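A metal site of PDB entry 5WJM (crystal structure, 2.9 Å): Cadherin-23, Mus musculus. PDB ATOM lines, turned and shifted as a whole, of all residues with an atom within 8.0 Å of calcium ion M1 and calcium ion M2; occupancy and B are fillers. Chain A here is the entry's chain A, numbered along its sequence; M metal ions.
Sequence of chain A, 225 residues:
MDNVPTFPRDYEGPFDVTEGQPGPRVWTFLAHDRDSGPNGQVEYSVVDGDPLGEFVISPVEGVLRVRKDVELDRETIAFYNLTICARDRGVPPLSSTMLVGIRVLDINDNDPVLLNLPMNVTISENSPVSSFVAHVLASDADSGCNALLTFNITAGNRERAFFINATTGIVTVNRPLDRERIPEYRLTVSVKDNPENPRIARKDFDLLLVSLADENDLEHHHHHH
OE1 of Glu 125 lies close to N of Arg 179 (2.9 Å).
OD2 of Asp 214 is in salt-bridge range of NH2 of Arg 179, 3.8 Å away.
OE1 of Glu 180 lies close to NH2 of Arg 179 (3.6 Å).
N of Glu 125 is in hydrogen-bond range of O of Ala 213 (3.3 Å).
Asn 216 touches calcium ion M1 (O to CA, 3.8 Å).
Within 4 Å of calcium ion M1: Glu 125, Glu 180, Asp 214, Glu 215, Asn 216 and Asp 217.
The nearest printed residue that does not touch calcium ion M1 is Arg 179 (4.7 Å).
Residues that only touch calcium ion M2: Asn 216.
Of the 12 residues printed, 5 come within 4 Å of calcium ion M2.
The nearest printed residue that does not touch calcium ion M2 is Asn 126 (4.4 Å).
Calcium ion M1 is bound by OE1 of Glu 180, OD1 of Asp 214, O of Glu 215, OD1 of Asp 217 and OE2 of Glu 125.
Calcium ion M2 is bound by OD1 of Asp 178 (2.3 Å), OD2 of Asp 217 (2.4 Å) and OE1 of Glu 125 (2.5 Å).
Slightly farther from calcium ion M2 lies OE2 of Glu 180 (3.0 Å).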
ATOM      1  N   GLU A 125     -12.824  15.828 -19.390  1.00  0.00           N
ATOM      2  CA  GLU A 125     -13.698  16.325 -18.317  1.00  0.00           C
ATOM      3  C   GLU A 125     -13.059  16.125 -16.938  1.00  0.00           C
ATOM      4  O   GLU A 125     -13.258  16.930 -16.014  1.00  0.00           O
ATOM      5  CB  GLU A 125     -15.110  15.716 -18.366  1.00  0.00           C
ATOM      6  CG  GLU A 125     -15.221  14.188 -18.296  1.00  0.00           C
ATOM      7  CD  GLU A 125     -16.621  13.690 -17.941  1.00  0.00           C
ATOM      8  OE1 GLU A 125     -17.394  14.436 -17.292  1.00  0.00           O
ATOM      9  OE2 GLU A 125     -16.969  12.524 -18.269  1.00  0.00           O
ATOM     10  N   ASN A 126     -12.260  15.065 -16.830  1.00  0.00           N
ATOM     11  CA  ASN A 126     -11.491  14.766 -15.621  1.00  0.00           C
ATOM     12  C   ASN A 126     -10.171  15.521 -15.533  1.00  0.00           C
ATOM     13  O   ASN A 126      -9.361  15.216 -14.658  1.00  0.00           O
ATOM     14  CB  ASN A 126     -11.210  13.258 -15.528  1.00  0.00           C
ATOM     15  CG  ASN A 126     -12.473  12.413 -15.465  1.00  0.00           C
ATOM     16  OD1 ASN A 126     -13.603  12.918 -15.403  1.00  0.00           O
ATOM     17  ND2 ASN A 126     -12.281  11.114 -15.491  1.00  0.00           N
ATOM     18  N   LEU A 177     -14.271  19.822 -13.319  1.00  0.00           N
ATOM     19  CA  LEU A 177     -15.134  19.910 -14.485  1.00  0.00           C
ATOM     20  C   LEU A 177     -15.997  18.650 -14.593  1.00  0.00           C
ATOM     21  O   LEU A 177     -15.536  17.567 -14.240  1.00  0.00           O
ATOM     22  CB  LEU A 177     -14.255  20.031 -15.734  1.00  0.00           C
ATOM     23  CG  LEU A 177     -13.823  21.401 -16.274  1.00  0.00           C
ATOM     24  CD1 LEU A 177     -13.383  22.372 -15.182  1.00  0.00           C
ATOM     25  CD2 LEU A 177     -12.711  21.206 -17.287  1.00  0.00           C
ATOM     26  N   ASP A 178     -17.233  18.787 -15.072  1.00  0.00           N
ATOM     27  CA  ASP A 178     -18.094  17.644 -15.449  1.00  0.00           C
ATOM     28  C   ASP A 178     -18.756  17.937 -16.790  1.00  0.00           C
ATOM     29  O   ASP A 178     -19.287  19.025 -17.008  1.00  0.00           O
ATOM     30  CB  ASP A 178     -19.155  17.383 -14.358  1.00  0.00           C
ATOM     31  CG  ASP A 178     -19.826  15.988 -14.454  1.00  0.00           C
ATOM     32  OD1 ASP A 178     -19.166  14.959 -14.738  1.00  0.00           O
ATOM     33  OD2 ASP A 178     -21.055  15.927 -14.184  1.00  0.00           O
ATOM     34  N   ARG A 179     -18.690  16.976 -17.710  1.00  0.00           N
ATOM     35  CA  ARG A 179     -19.272  17.156 -19.034  1.00  0.00           C
ATOM     36  C   ARG A 179     -20.792  17.068 -18.986  1.00  0.00           C
ATOM     37  O   ARG A 179     -21.468  17.610 -19.847  1.00  0.00           O
ATOM     38  CB  ARG A 179     -18.750  16.111 -20.015  1.00  0.00           C
ATOM     39  CG  ARG A 179     -18.934  16.514 -21.477  1.00  0.00           C
ATOM     40  CD  ARG A 179     -18.423  15.432 -22.430  1.00  0.00           C
ATOM     41  NE  ARG A 179     -19.195  14.204 -22.241  1.00  0.00           N
ATOM     42  CZ  ARG A 179     -20.431  14.008 -22.688  1.00  0.00           C
ATOM     43  NH1 ARG A 179     -21.068  14.939 -23.396  1.00  0.00           N
ATOM     44  NH2 ARG A 179     -21.046  12.854 -22.426  1.00  0.00           N
ATOM     45  N   GLU A 180     -21.310  16.375 -17.998  1.00  0.00           N
ATOM     46  CA  GLU A 180     -22.743  16.152 -17.903  1.00  0.00           C
ATOM     47  C   GLU A 180     -23.435  17.381 -17.331  1.00  0.00           C
ATOM     48  O   GLU A 180     -24.615  17.594 -17.599  1.00  0.00           O
ATOM     49  CB  GLU A 180     -23.051  14.878 -17.101  1.00  0.00           C
ATOM     50  CG  GLU A 180     -22.668  13.555 -17.788  1.00  0.00           C
ATOM     51  CD  GLU A 180     -21.159  13.274 -17.815  1.00  0.00           C
ATOM     52  OE1 GLU A 180     -20.675  12.697 -18.811  1.00  0.00           O
ATOM     53  OE2 GLU A 180     -20.441  13.614 -16.836  1.00  0.00           O
ATOM     54  N   ARG A 181     -22.713  18.194 -16.550  1.00  0.00           N
ATOM     55  CA  ARG A 181     -23.188  19.535 -16.145  1.00  0.00           C
ATOM     56  C   ARG A 181     -23.007  20.545 -17.260  1.00  0.00           C
ATOM     57  O   ARG A 181     -23.970  21.121 -17.708  1.00  0.00           O
ATOM     58  CB  ARG A 181     -22.444  20.070 -14.924  1.00  0.00           C
ATOM     59  CG  ARG A 181     -22.687  19.309 -13.629  1.00  0.00           C
ATOM     60  CD  ARG A 181     -21.988  20.014 -12.469  1.00  0.00           C
ATOM     61  NE  ARG A 181     -22.373  21.416 -12.420  1.00  0.00           N
ATOM     62  CZ  ARG A 181     -23.531  21.877 -11.930  1.00  0.00           C
ATOM     63  NH1 ARG A 181     -23.775  23.183 -11.955  1.00  0.00           N
ATOM     64  NH2 ARG A 181     -24.448  21.054 -11.414  1.00  0.00           N
ATOM     65  N   ALA A 213     -14.094  16.377 -23.553  1.00  0.00           N
ATOM     66  CA  ALA A 213     -14.229  14.987 -23.996  1.00  0.00           C
ATOM     67  C   ALA A 213     -14.855  14.084 -22.912  1.00  0.00           C
ATOM     68  O   ALA A 213     -14.533  14.246 -21.729  1.00  0.00           O
ATOM     69  CB  ALA A 213     -12.872  14.439 -24.378  1.00  0.00           C
ATOM     70  N   ASP A 214     -15.688  13.132 -23.308  1.00  0.00           N
ATOM     71  CA  ASP A 214     -16.337  12.243 -22.328  1.00  0.00           C
ATOM     72  C   ASP A 214     -15.331  11.297 -21.642  1.00  0.00           C
ATOM     73  O   ASP A 214     -14.284  10.973 -22.197  1.00  0.00           O
ATOM     74  CB  ASP A 214     -17.495  11.423 -22.938  1.00  0.00           C
ATOM     75  CG  ASP A 214     -18.482  10.863 -21.858  1.00  0.00           C
ATOM     76  OD1 ASP A 214     -18.849  11.590 -20.903  1.00  0.00           O
ATOM     77  OD2 ASP A 214     -18.913   9.702 -21.960  1.00  0.00           O
ATOM     78  N   GLU A 215     -15.662  10.941 -20.392  1.00  0.00           N
ATOM     79  CA  GLU A 215     -14.995   9.893 -19.604  1.00  0.00           C
ATOM     80  C   GLU A 215     -16.051   9.175 -18.736  1.00  0.00           C
ATOM     81  O   GLU A 215     -17.252   9.492 -18.813  1.00  0.00           O
ATOM     82  CB  GLU A 215     -13.892  10.510 -18.708  1.00  0.00           C
ATOM     83  CG  GLU A 215     -12.750  11.244 -19.410  1.00  0.00           C
ATOM     84  CD  GLU A 215     -11.756  10.315 -20.100  1.00  0.00           C
ATOM     85  OE1 GLU A 215     -12.178   9.304 -20.715  1.00  0.00           O
ATOM     86  OE2 GLU A 215     -10.535  10.592 -20.051  1.00  0.00           O
ATOM     87  N   ASN A 216     -15.602   8.233 -17.907  1.00  0.00           N
ATOM     88  CA  ASN A 216     -16.482   7.519 -16.967  1.00  0.00           C
ATOM     89  C   ASN A 216     -17.097   8.413 -15.889  1.00  0.00           C
ATOM     90  O   ASN A 216     -16.795   9.624 -15.832  1.00  0.00           O
ATOM     91  CB  ASN A 216     -15.736   6.360 -16.289  1.00  0.00           C
ATOM     92  CG  ASN A 216     -15.414   5.238 -17.249  1.00  0.00           C
ATOM     93  OD1 ASN A 216     -15.762   5.298 -18.427  1.00  0.00           O
ATOM     94  ND2 ASN A 216     -14.730   4.201 -16.750  1.00  0.00           N
ATOM     95  N   ASP A 217     -17.984   7.804 -15.088  1.00  0.00           N
ATOM     96  CA  ASP A 217     -18.673   8.450 -13.967  1.00  0.00           C
ATOM     97  C   ASP A 217     -18.959   7.412 -12.872  1.00  0.00           C
ATOM     98  O   ASP A 217     -18.353   7.437 -11.807  1.00  0.00           O
ATOM     99  CB  ASP A 217     -19.998   9.077 -14.449  1.00  0.00           C
ATOM    100  CG  ASP A 217     -19.802  10.109 -15.588  1.00  0.00           C
ATOM    101  OD1 ASP A 217     -19.788   9.723 -16.779  1.00  0.00           O
ATOM    102  OD2 ASP A 217     -19.649  11.319 -15.292  1.00  0.00           O
HETATM  103 CA    CA M   1     -19.022  11.059 -18.601  1.00  0.00          CA
HETATM  104 CA    CA M   2     -17.980  13.063 -15.249  1.00  0.00          CA
